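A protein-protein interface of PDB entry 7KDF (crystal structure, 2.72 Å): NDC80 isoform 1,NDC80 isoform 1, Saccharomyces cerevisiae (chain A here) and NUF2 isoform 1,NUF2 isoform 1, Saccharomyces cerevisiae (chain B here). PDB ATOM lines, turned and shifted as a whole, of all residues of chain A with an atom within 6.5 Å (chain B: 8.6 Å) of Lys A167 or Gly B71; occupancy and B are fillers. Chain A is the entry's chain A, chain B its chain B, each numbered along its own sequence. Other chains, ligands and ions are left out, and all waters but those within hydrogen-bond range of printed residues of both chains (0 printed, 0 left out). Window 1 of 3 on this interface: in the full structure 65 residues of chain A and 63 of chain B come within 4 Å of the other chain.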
ATOM      1  N   GLN A 136     -33.966  23.633 -18.627  1.00  0.00           N
ATOM      2  CA  GLN A 136     -33.435  22.425 -18.003  1.00  0.00           C
ATOM      3  C   GLN A 136     -31.992  22.590 -17.552  1.00  0.00           C
ATOM      4  O   GLN A 136     -31.547  21.854 -16.669  1.00  0.00           O
ATOM      5  CB  GLN A 136     -33.541  21.235 -18.959  1.00  0.00           C
ATOM      6  CG  GLN A 136     -34.959  20.770 -19.180  1.00  0.00           C
ATOM      7  CD  GLN A 136     -35.036  19.376 -19.749  1.00  0.00           C
ATOM      8  OE1 GLN A 136     -34.170  18.539 -19.492  1.00  0.00           O
ATOM      9  NE2 GLN A 136     -36.083  19.112 -20.523  1.00  0.00           N
ATOM     10  N   ASN A 137     -31.260  23.547 -18.122  1.00  0.00           N
ATOM     11  CA  ASN A 137     -29.879  23.756 -17.720  1.00  0.00           C
ATOM     12  C   ASN A 137     -29.771  24.347 -16.322  1.00  0.00           C
ATOM     13  O   ASN A 137     -28.678  24.379 -15.759  1.00  0.00           O
ATOM     14  CB  ASN A 137     -29.178  24.671 -18.722  1.00  0.00           C
ATOM     15  CG  ASN A 137     -27.666  24.596 -18.627  1.00  0.00           C
ATOM     16  OD1 ASN A 137     -26.992  25.614 -18.437  1.00  0.00           O
ATOM     17  ND2 ASN A 137     -27.124  23.386 -18.740  1.00  0.00           N
ATOM     18  N   THR A 138     -30.869  24.817 -15.737  1.00  0.00           N
ATOM     19  CA  THR A 138     -30.816  25.490 -14.435  1.00  0.00           C
ATOM     20  C   THR A 138     -31.650  24.825 -13.352  1.00  0.00           C
ATOM     21  O   THR A 138     -31.777  25.388 -12.234  1.00  0.00           O
ATOM     22  CB  THR A 138     -31.304  26.934 -14.542  1.00  0.00           C
ATOM     23  OG1 THR A 138     -32.742  26.928 -14.570  1.00  0.00           O
ATOM     24  CG2 THR A 138     -30.750  27.602 -15.766  1.00  0.00           C
ATOM     25  N   GLN A 139     -32.258  23.677 -13.662  1.00  0.00           N
ATOM     26  CA  GLN A 139     -33.277  23.140 -12.767  1.00  0.00           C
ATOM     27  C   GLN A 139     -32.649  22.776 -11.411  1.00  0.00           C
ATOM     28  O   GLN A 139     -33.147  23.133 -10.327  1.00  0.00           O
ATOM     29  CB  GLN A 139     -33.922  21.888 -13.364  1.00  0.00           C
ATOM     30  CG  GLN A 139     -34.544  21.933 -14.686  1.00  0.00           C
ATOM     31  CD  GLN A 139     -35.296  20.666 -14.893  1.00  0.00           C
ATOM     32  OE1 GLN A 139     -35.357  19.786 -13.942  1.00  0.00           O
ATOM     33  NE2 GLN A 139     -35.786  20.497 -16.142  1.00  0.00           N
ATOM     34  N   GLU A 140     -31.492  22.121 -11.491  1.00  0.00           N
ATOM     35  CA  GLU A 140     -30.807  21.576 -10.335  1.00  0.00           C
ATOM     36  C   GLU A 140     -30.381  22.669  -9.377  1.00  0.00           C
ATOM     37  O   GLU A 140     -30.703  22.616  -8.187  1.00  0.00           O
ATOM     38  CB  GLU A 140     -29.587  20.789 -10.804  1.00  0.00           C
ATOM     39  CG  GLU A 140     -29.853  19.491 -11.577  1.00  0.00           C
ATOM     40  CD  GLU A 140     -30.116  19.703 -13.063  1.00  0.00           C
ATOM     41  OE1 GLU A 140     -30.780  18.830 -13.671  1.00  0.00           O
ATOM     42  OE2 GLU A 140     -29.650  20.729 -13.625  1.00  0.00           O
ATOM     43  N   GLU A 162     -25.015  15.134  -8.639  1.00  0.00           N
ATOM     44  CA  GLU A 162     -24.199  14.424  -9.615  1.00  0.00           C
ATOM     45  C   GLU A 162     -24.622  14.768 -11.034  1.00  0.00           C
ATOM     46  O   GLU A 162     -23.779  14.881 -11.931  1.00  0.00           O
ATOM     47  CB  GLU A 162     -24.276  12.919  -9.365  1.00  0.00           C
ATOM     48  CG  GLU A 162     -23.725  12.513  -8.010  1.00  0.00           C
ATOM     49  CD  GLU A 162     -23.964  11.049  -7.685  1.00  0.00           C
ATOM     50  OE1 GLU A 162     -23.037  10.404  -7.150  1.00  0.00           O
ATOM     51  OE2 GLU A 162     -25.076  10.547  -7.959  1.00  0.00           O
ATOM     52  N   LEU A 163     -25.926  14.954 -11.256  1.00  0.00           N
ATOM     53  CA  LEU A 163     -26.389  15.357 -12.579  1.00  0.00           C
ATOM     54  C   LEU A 163     -25.866  16.744 -12.936  1.00  0.00           C
ATOM     55  O   LEU A 163     -25.467  16.988 -14.079  1.00  0.00           O
ATOM     56  CB  LEU A 163     -27.916  15.323 -12.641  1.00  0.00           C
ATOM     57  CG  LEU A 163     -28.562  15.728 -13.967  1.00  0.00           C
ATOM     58  CD1 LEU A 163     -27.963  14.935 -15.120  1.00  0.00           C
ATOM     59  CD2 LEU A 163     -30.074  15.587 -13.920  1.00  0.00           C
ATOM     60  N   MET A 164     -25.855  17.665 -11.968  1.00  0.00           N
ATOM     61  CA  MET A 164     -25.346  19.008 -12.237  1.00  0.00           C
ATOM     62  C   MET A 164     -23.874  18.979 -12.631  1.00  0.00           C
ATOM     63  O   MET A 164     -23.471  19.649 -13.587  1.00  0.00           O
ATOM     64  CB  MET A 164     -25.589  19.909 -11.027  1.00  0.00           C
ATOM     65  CG  MET A 164     -25.111  21.347 -11.185  1.00  0.00           C
ATOM     66  SD  MET A 164     -25.519  22.337  -9.723  1.00  0.00           S
ATOM     67  CE  MET A 164     -24.403  21.641  -8.536  1.00  0.00           C
ATOM     68  N   VAL A 165     -23.066  18.171 -11.942  1.00  0.00           N
ATOM     69  CA  VAL A 165     -21.655  18.065 -12.294  1.00  0.00           C
ATOM     70  C   VAL A 165     -21.494  17.356 -13.635  1.00  0.00           C
ATOM     71  O   VAL A 165     -20.624  17.711 -14.439  1.00  0.00           O
ATOM     72  CB  VAL A 165     -20.874  17.367 -11.164  1.00  0.00           C
ATOM     73  CG1 VAL A 165     -19.526  16.844 -11.659  1.00  0.00           C
ATOM     74  CG2 VAL A 165     -20.672  18.324 -10.000  1.00  0.00           C
ATOM     75  N   GLU A 166     -22.334  16.355 -13.909  1.00  0.00           N
ATOM     76  CA  GLU A 166     -22.237  15.669 -15.191  1.00  0.00           C
ATOM     77  C   GLU A 166     -22.585  16.602 -16.344  1.00  0.00           C
ATOM     78  O   GLU A 166     -21.964  16.526 -17.411  1.00  0.00           O
ATOM     79  CB  GLU A 166     -23.127  14.427 -15.205  1.00  0.00           C
ATOM     80  CG  GLU A 166     -22.986  13.579 -16.469  1.00  0.00           C
ATOM     81  CD  GLU A 166     -21.533  13.273 -16.829  1.00  0.00           C
ATOM     82  OE1 GLU A 166     -20.734  12.977 -15.914  1.00  0.00           O
ATOM     83  OE2 GLU A 166     -21.194  13.327 -18.033  1.00  0.00           O
ATOM     84  N   LYS A 167     -23.562  17.493 -16.155  1.00  0.00           N
ATOM     85  CA  LYS A 167     -23.888  18.451 -17.208  1.00  0.00           C
ATOM     86  C   LYS A 167     -22.743  19.426 -17.460  1.00  0.00           C
ATOM     87  O   LYS A 167     -22.591  19.927 -18.581  1.00  0.00           O
ATOM     88  CB  LYS A 167     -25.163  19.219 -16.864  1.00  0.00           C
ATOM     89  CG  LYS A 167     -26.440  18.464 -17.183  1.00  0.00           C
ATOM     90  CD  LYS A 167     -27.657  19.233 -16.701  1.00  0.00           C
ATOM     91  CE  LYS A 167     -28.944  18.542 -17.101  1.00  0.00           C
ATOM     92  NZ  LYS A 167     -30.132  19.288 -16.608  1.00  0.00           N
ATOM     93  N   LEU A 168     -21.945  19.725 -16.434  1.00  0.00           N
ATOM     94  CA  LEU A 168     -20.790  20.590 -16.638  1.00  0.00           C
ATOM     95  C   LEU A 168     -19.745  19.893 -17.498  1.00  0.00           C
ATOM     96  O   LEU A 168     -19.194  20.488 -18.433  1.00  0.00           O
ATOM     97  CB  LEU A 168     -20.193  20.995 -15.294  1.00  0.00           C
ATOM     98  CG  LEU A 168     -20.988  21.979 -14.440  1.00  0.00           C
ATOM     99  CD1 LEU A 168     -20.309  22.155 -13.084  1.00  0.00           C
ATOM    100  CD2 LEU A 168     -21.141  23.313 -15.160  1.00  0.00           C
ATOM    101  N   LEU A 169     -19.467  18.623 -17.194  1.00  0.00           N
ATOM    102  CA  LEU A 169     -18.513  17.862 -17.991  1.00  0.00           C
ATOM    103  C   LEU A 169     -19.022  17.659 -19.413  1.00  0.00           C
ATOM    104  O   LEU A 169     -18.248  17.735 -20.374  1.00  0.00           O
ATOM    105  CB  LEU A 169     -18.225  16.525 -17.316  1.00  0.00           C
ATOM    106  CG  LEU A 169     -17.604  16.596 -15.920  1.00  0.00           C
ATOM    107  CD1 LEU A 169     -17.164  15.221 -15.459  1.00  0.00           C
ATOM    108  CD2 LEU A 169     -16.439  17.559 -15.892  1.00  0.00           C
ATOM    109  N   ILE A 170     -20.327  17.415 -19.567  1.00  0.00           N
ATOM    110  CA  ILE A 170     -20.902  17.278 -20.902  1.00  0.00           C
ATOM    111  C   ILE A 170     -20.666  18.547 -21.711  1.00  0.00           C
ATOM    112  O   ILE A 170     -20.339  18.490 -22.903  1.00  0.00           O
ATOM    113  CB  ILE A 170     -22.399  16.933 -20.809  1.00  0.00           C
ATOM    114  CG1 ILE A 170     -22.587  15.488 -20.342  1.00  0.00           C
ATOM    115  CG2 ILE A 170     -23.089  17.161 -22.143  1.00  0.00           C
ATOM    116  CD1 ILE A 170     -24.030  15.109 -20.108  1.00  0.00           C
ATOM    117  N   ASP A 171     -20.815  19.711 -21.078  1.00  0.00           N
ATOM    118  CA  ASP A 171     -20.517  20.962 -21.763  1.00  0.00           C
ATOM    119  C   ASP A 171     -19.054  21.028 -22.173  1.00  0.00           C
ATOM    120  O   ASP A 171     -18.733  21.431 -23.297  1.00  0.00           O
ATOM    121  CB  ASP A 171     -20.858  22.151 -20.868  1.00  0.00           C
ATOM    122  CG  ASP A 171     -22.340  22.360 -20.724  1.00  0.00           C
ATOM    123  OD1 ASP A 171     -22.730  23.232 -19.916  1.00  0.00           O
ATOM    124  OD2 ASP A 171     -23.107  21.659 -21.423  1.00  0.00           O
ATOM    125  N   TYR A 172     -18.155  20.644 -21.267  1.00  0.00           N
ATOM    126  CA  TYR A 172     -16.731  20.751 -21.553  1.00  0.00           C
ATOM    127  C   TYR A 172     -16.346  19.896 -22.752  1.00  0.00           C
ATOM    128  O   TYR A 172     -15.745  20.383 -23.714  1.00  0.00           O
ATOM    129  CB  TYR A 172     -15.923  20.343 -20.324  1.00  0.00           C
ATOM    130  CG  TYR A 172     -14.454  20.219 -20.612  1.00  0.00           C
ATOM    131  CD1 TYR A 172     -13.708  21.331 -20.968  1.00  0.00           C
ATOM    132  CD2 TYR A 172     -13.812  18.987 -20.544  1.00  0.00           C
ATOM    133  CE1 TYR A 172     -12.360  21.226 -21.240  1.00  0.00           C
ATOM    134  CE2 TYR A 172     -12.460  18.873 -20.816  1.00  0.00           C
ATOM    135  CZ  TYR A 172     -11.740  19.999 -21.164  1.00  0.00           C
ATOM    136  OH  TYR A 172     -10.397  19.908 -21.436  1.00  0.00           O
ATOM    137  N   LYS B  63     -32.212   7.300 -29.293  1.00  0.00           N
ATOM    138  CA  LYS B  63     -32.708   7.971 -28.095  1.00  0.00           C
ATOM    139  C   LYS B  63     -31.832   7.653 -26.893  1.00  0.00           C
ATOM    140  O   LYS B  63     -31.521   8.537 -26.085  1.00  0.00           O
ATOM    141  CB  LYS B  63     -34.159   7.577 -27.826  1.00  0.00           C
ATOM    142  CG  LYS B  63     -35.158   8.221 -28.774  1.00  0.00           C
ATOM    143  CD  LYS B  63     -36.500   8.465 -28.109  1.00  0.00           C
ATOM    144  CE  LYS B  63     -37.511   7.404 -28.482  1.00  0.00           C
ATOM    145  NZ  LYS B  63     -38.728   7.513 -27.632  1.00  0.00           N
ATOM    146  N   GLN B  64     -31.405   6.399 -26.767  1.00  0.00           N
ATOM    147  CA  GLN B  64     -30.536   6.043 -25.653  1.00  0.00           C
ATOM    148  C   GLN B  64     -29.190   6.756 -25.749  1.00  0.00           C
ATOM    149  O   GLN B  64     -28.674   7.255 -24.742  1.00  0.00           O
ATOM    150  CB  GLN B  64     -30.356   4.531 -25.607  1.00  0.00           C
ATOM    151  CG  GLN B  64     -29.783   4.006 -24.313  1.00  0.00           C
ATOM    152  CD  GLN B  64     -29.633   2.498 -24.331  1.00  0.00           C
ATOM    153  OE1 GLN B  64     -30.147   1.821 -25.226  1.00  0.00           O
ATOM    154  NE2 GLN B  64     -28.928   1.962 -23.342  1.00  0.00           N
ATOM    155  N   ILE B  65     -28.613   6.825 -26.951  1.00  0.00           N
ATOM    156  CA  ILE B  65     -27.308   7.462 -27.123  1.00  0.00           C
ATOM    157  C   ILE B  65     -27.396   8.950 -26.809  1.00  0.00           C
ATOM    158  O   ILE B  65     -26.576   9.496 -26.059  1.00  0.00           O
ATOM    159  CB  ILE B  65     -26.783   7.232 -28.550  1.00  0.00           C
ATOM    160  CG1 ILE B  65     -26.362   5.778 -28.748  1.00  0.00           C
ATOM    161  CG2 ILE B  65     -25.634   8.178 -28.859  1.00  0.00           C
ATOM    162  CD1 ILE B  65     -26.343   5.366 -30.199  1.00  0.00           C
ATOM    163  N   ILE B  66     -28.394   9.625 -27.379  1.00  0.00           N
ATOM    164  CA  ILE B  66     -28.525  11.066 -27.183  1.00  0.00           C
ATOM    165  C   ILE B  66     -28.783  11.390 -25.717  1.00  0.00           C
ATOM    166  O   ILE B  66     -28.211  12.339 -25.167  1.00  0.00           O
ATOM    167  CB  ILE B  66     -29.625  11.624 -28.102  1.00  0.00           C
ATOM    168  CG1 ILE B  66     -29.095  11.718 -29.530  1.00  0.00           C
ATOM    169  CG2 ILE B  66     -30.064  12.987 -27.639  1.00  0.00           C
ATOM    170  CD1 ILE B  66     -30.172  11.748 -30.566  1.00  0.00           C
ATOM    171  N   GLU B  67     -29.637  10.609 -25.055  1.00  0.00           N
ATOM    172  CA  GLU B  67     -29.914  10.894 -23.653  1.00  0.00           C
ATOM    173  C   GLU B  67     -28.677  10.694 -22.786  1.00  0.00           C
ATOM    174  O   GLU B  67     -28.501  11.407 -21.793  1.00  0.00           O
ATOM    175  CB  GLU B  67     -31.076  10.037 -23.163  1.00  0.00           C
ATOM    176  CG  GLU B  67     -32.399  10.462 -23.785  1.00  0.00           C
ATOM    177  CD  GLU B  67     -33.587   9.702 -23.240  1.00  0.00           C
ATOM    178  OE1 GLU B  67     -33.379   8.670 -22.567  1.00  0.00           O
ATOM    179  OE2 GLU B  67     -34.729  10.144 -23.493  1.00  0.00           O
ATOM    180  N   ASN B  68     -27.799   9.761 -23.157  1.00  0.00           N
ATOM    181  CA  ASN B  68     -26.594   9.532 -22.365  1.00  0.00           C
ATOM    182  C   ASN B  68     -25.579  10.653 -22.557  1.00  0.00           C
ATOM    183  O   ASN B  68     -25.076  11.222 -21.581  1.00  0.00           O
ATOM    184  CB  ASN B  68     -25.967   8.187 -22.732  1.00  0.00           C
ATOM    185  CG  ASN B  68     -24.849   7.793 -21.787  1.00  0.00           C
ATOM    186  OD1 ASN B  68     -23.692   7.657 -22.192  1.00  0.00           O
ATOM    187  ND2 ASN B  68     -25.188   7.609 -20.516  1.00  0.00           N
ATOM    188  N   PHE B  69     -25.263  10.984 -23.809  1.00  0.00           N
ATOM    189  CA  PHE B  69     -24.167  11.902 -24.085  1.00  0.00           C
ATOM    190  C   PHE B  69     -24.548  13.357 -23.865  1.00  0.00           C
ATOM    191  O   PHE B  69     -23.665  14.184 -23.614  1.00  0.00           O
ATOM    192  CB  PHE B  69     -23.654  11.699 -25.515  1.00  0.00           C
ATOM    193  CG  PHE B  69     -22.825  10.450 -25.694  1.00  0.00           C
ATOM    194  CD1 PHE B  69     -22.484   9.663 -24.608  1.00  0.00           C
ATOM    195  CD2 PHE B  69     -22.386  10.065 -26.948  1.00  0.00           C
ATOM    196  CE1 PHE B  69     -21.726   8.516 -24.771  1.00  0.00           C
ATOM    197  CE2 PHE B  69     -21.625   8.919 -27.113  1.00  0.00           C
ATOM    198  CZ  PHE B  69     -21.296   8.147 -26.024  1.00  0.00           C
ATOM    199  N   MET B  70     -25.833  13.689 -23.936  1.00  0.00           N
ATOM    200  CA  MET B  70     -26.286  15.047 -23.679  1.00  0.00           C
ATOM    201  C   MET B  70     -26.906  15.236 -22.306  1.00  0.00           C
ATOM    202  O   MET B  70     -27.094  16.380 -21.883  1.00  0.00           O
ATOM    203  CB  MET B  70     -27.306  15.469 -24.730  1.00  0.00           C
ATOM    204  CG  MET B  70     -26.744  15.721 -26.103  1.00  0.00           C
ATOM    205  SD  MET B  70     -28.149  16.050 -27.203  1.00  0.00           S
ATOM    206  CE  MET B  70     -28.871  17.541 -26.557  1.00  0.00           C
ATOM    207  N   GLY B  71     -27.247  14.156 -21.616  1.00  0.00           N
ATOM    208  CA  GLY B  71     -27.804  14.291 -20.286  1.00  0.00           C
ATOM    209  C   GLY B  71     -29.155  14.970 -20.231  1.00  0.00           C
ATOM    210  O   GLY B  71     -29.435  15.698 -19.273  1.00  0.00           O
ATOM    211  N   ILE B  72     -30.008  14.746 -21.229  1.00  0.00           N
ATOM    212  CA  ILE B  72     -31.348  15.311 -21.235  1.00  0.00           C
ATOM    213  C   ILE B  72     -32.337  14.188 -21.499  1.00  0.00           C
ATOM    214  O   ILE B  72     -31.984  13.114 -21.989  1.00  0.00           O
ATOM    215  CB  ILE B  72     -31.544  16.383 -22.312  1.00  0.00           C
ATOM    216  CG1 ILE B  72     -31.536  15.688 -23.672  1.00  0.00           C
ATOM    217  CG2 ILE B  72     -30.442  17.428 -22.224  1.00  0.00           C
ATOM    218  CD1 ILE B  72     -31.945  16.562 -24.802  1.00  0.00           C
ATOM    219  N   SER B  73     -33.598  14.469 -21.199  1.00  0.00           N
ATOM    220  CA  SER B  73     -34.688  13.559 -21.513  1.00  0.00           C
ATOM    221  C   SER B  73     -35.284  13.951 -22.857  1.00  0.00           C
ATOM    222  O   SER B  73     -35.796  15.066 -23.015  1.00  0.00           O
ATOM    223  CB  SER B  73     -35.760  13.595 -20.430  1.00  0.00           C
ATOM    224  OG  SER B  73     -36.866  12.806 -20.822  1.00  0.00           O
ATOM    225  N   VAL B  74     -35.224  13.033 -23.820  1.00  0.00           N
ATOM    226  CA  VAL B  74     -35.909  13.262 -25.086  1.00  0.00           C
ATOM    227  C   VAL B  74     -37.406  13.424 -24.847  1.00  0.00           C
ATOM    228  O   VAL B  74     -38.045  14.320 -25.412  1.00  0.00           O
ATOM    229  CB  VAL B  74     -35.595  12.123 -26.075  1.00  0.00           C
ATOM    230  CG1 VAL B  74     -36.567  12.126 -27.236  1.00  0.00           C
ATOM    231  CG2 VAL B  74     -34.174  12.254 -26.587  1.00  0.00           C
ATOM    232  N   SER B  76     -39.008  14.617 -22.243  1.00  0.00           N
ATOM    233  CA  SER B  76     -39.323  15.948 -21.734  1.00  0.00           C
ATOM    234  C   SER B  76     -39.291  16.989 -22.841  1.00  0.00           C
ATOM    235  O   SER B  76     -40.055  17.961 -22.806  1.00  0.00           O
ATOM    236  CB  SER B  76     -38.354  16.338 -20.616  1.00  0.00           C
ATOM    237  OG  SER B  76     -37.076  16.661 -21.140  1.00  0.00           O
ATOM    238  N   PHE B 114     -27.597  16.971 -32.478  1.00  0.00           N
ATOM    239  CA  PHE B 114     -26.595  16.174 -31.781  1.00  0.00           C
ATOM    240  C   PHE B 114     -25.483  15.734 -32.723  1.00  0.00           C
ATOM    241  O   PHE B 114     -24.298  15.809 -32.377  1.00  0.00           O
ATOM    242  CB  PHE B 114     -27.253  14.958 -31.136  1.00  0.00           C
ATOM    243  CG  PHE B 114     -26.276  13.911 -30.691  1.00  0.00           C
ATOM    244  CD1 PHE B 114     -25.553  14.072 -29.521  1.00  0.00           C
ATOM    245  CD2 PHE B 114     -26.075  12.768 -31.444  1.00  0.00           C
ATOM    246  CE1 PHE B 114     -24.656  13.108 -29.103  1.00  0.00           C
ATOM    247  CE2 PHE B 114     -25.175  11.799 -31.031  1.00  0.00           C
ATOM    248  CZ  PHE B 114     -24.468  11.970 -29.858  1.00  0.00           C
ATOM    249  N   TYR B 146     -16.499  10.093 -30.666  1.00  0.00           N
ATOM    250  CA  TYR B 146     -16.727  11.056 -29.592  1.00  0.00           C
ATOM    251  C   TYR B 146     -16.507  10.420 -28.221  1.00  0.00           C
ATOM    252  O   TYR B 146     -15.897  11.033 -27.334  1.00  0.00           O
ATOM    253  CB  TYR B 146     -18.132  11.646 -29.698  1.00  0.00           C
ATOM    254  CG  TYR B 146     -18.511  12.494 -28.509  1.00  0.00           C
ATOM    255  CD1 TYR B 146     -17.862  13.694 -28.250  1.00  0.00           C
ATOM    256  CD2 TYR B 146     -19.503  12.085 -27.630  1.00  0.00           C
ATOM    257  CE1 TYR B 146     -18.198  14.468 -27.149  1.00  0.00           C
ATOM    258  CE2 TYR B 146     -19.842  12.849 -26.531  1.00  0.00           C
ATOM    259  CZ  TYR B 146     -19.189  14.039 -26.294  1.00  0.00           C
ATOM    260  OH  TYR B 146     -19.537  14.798 -25.198  1.00  0.00           O
ATOM    261  N   ARG B 150     -13.848  11.481 -25.266  1.00  0.00           N
ATOM    262  CA  ARG B 150     -14.206  11.789 -23.886  1.00  0.00           C
ATOM    263  C   ARG B 150     -13.392  10.955 -22.902  1.00  0.00           C
ATOM    264  O   ARG B 150     -12.917  11.471 -21.882  1.00  0.00           O
ATOM    265  CB  ARG B 150     -15.689  11.547 -23.654  1.00  0.00           C
ATOM    266  CG  ARG B 150     -16.098  12.041 -22.308  1.00  0.00           C
ATOM    267  CD  ARG B 150     -17.600  11.835 -22.017  1.00  0.00           C
ATOM    268  NE  ARG B 150     -17.815  12.340 -20.673  1.00  0.00           N
ATOM    269  CZ  ARG B 150     -18.141  13.595 -20.371  1.00  0.00           C
ATOM    270  NH1 ARG B 150     -18.323  13.918 -19.096  1.00  0.00           N
ATOM    271  NH2 ARG B 150     -18.261  14.535 -21.308  1.00  0.00           N
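NH2 of Arg B150 lies within hydrogen-bond range of O of Leu A169, at 3.3 Å. The guanidinium group (NH1) of Arg B150 lies within salt-bridge range of the side-chain carboxylate (OE2) of Glu A166, 3.1 Å away. The side-chain amide nitrogen (NE2) of Gln A136 is in hydrogen-bond range of the side-chain hydroxyl (OG) of Ser B76, 2.7 Å away.
The side-chain carboxylate (OE1) of Glu A140 lies within salt-bridge range of the side-chain amino group (NZ) of Lys A167, 3.0 Å away. O of Gln A136 lies within hydrogen-bond range of NZ of Lys A167 (2.9 Å). The side-chain hydroxyl (OG) of Ser B76 lies within hydrogen-bond range of the backbone carbonyl oxygen (O) of Ser B73, at 2.8 Å.
Lys A167 touches Gly B71. Ile A170 touches Phe B69 (CG2 to O, 3.4 Å). Met B70 touches Ile A170 (C to CD1, 3.6 Å). CD1 of Ile A170 touches N of Gly B71, at 3.7 Å. Ile A170 touches Arg B150.
Lys A167 touches just one residue of chain B: Gly B71 (3.6 Å). Gly B71 touches just these residues of chain A: Lys A167 and Ile A170. Printed residues of chain A within 4 Å of Arg B150: Glu A166 (3.1 Å), Leu A169 (3.2 Å) and Ile A170 (3.8 Å). Printed residues of chain B within 4 Å of Ile A170: Phe B69 (3.4 Å), Met B70 (3.6 Å), Gly B71 (3.7 Å) and Arg B150 (3.8 Å). Printed residues of chain A within 4 Å of Ser B76: Gln A136. Printed residues of chain B within 4 Å of Gln A136: Ser B76. Of the printed residues of chain A, Phe B69 touches Ile A170 (3.4 Å).
Of the 16 printed residues of chain A, 5 touch a printed residue of chain B. Printed residues of chain A that touch a printed residue of chain B: Gln A136, Glu A166, Lys A167, Leu A169 and Ile A170. Along chain B the printed residues that touch a printed residue of chain A span positions 69 to 150. Among the printed residues, Asp or Glu carboxylates within 4 Å of a Lys or Arg side-chain nitrogen of the other chain: Glu A166 with Arg B150 (3.1 Å).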
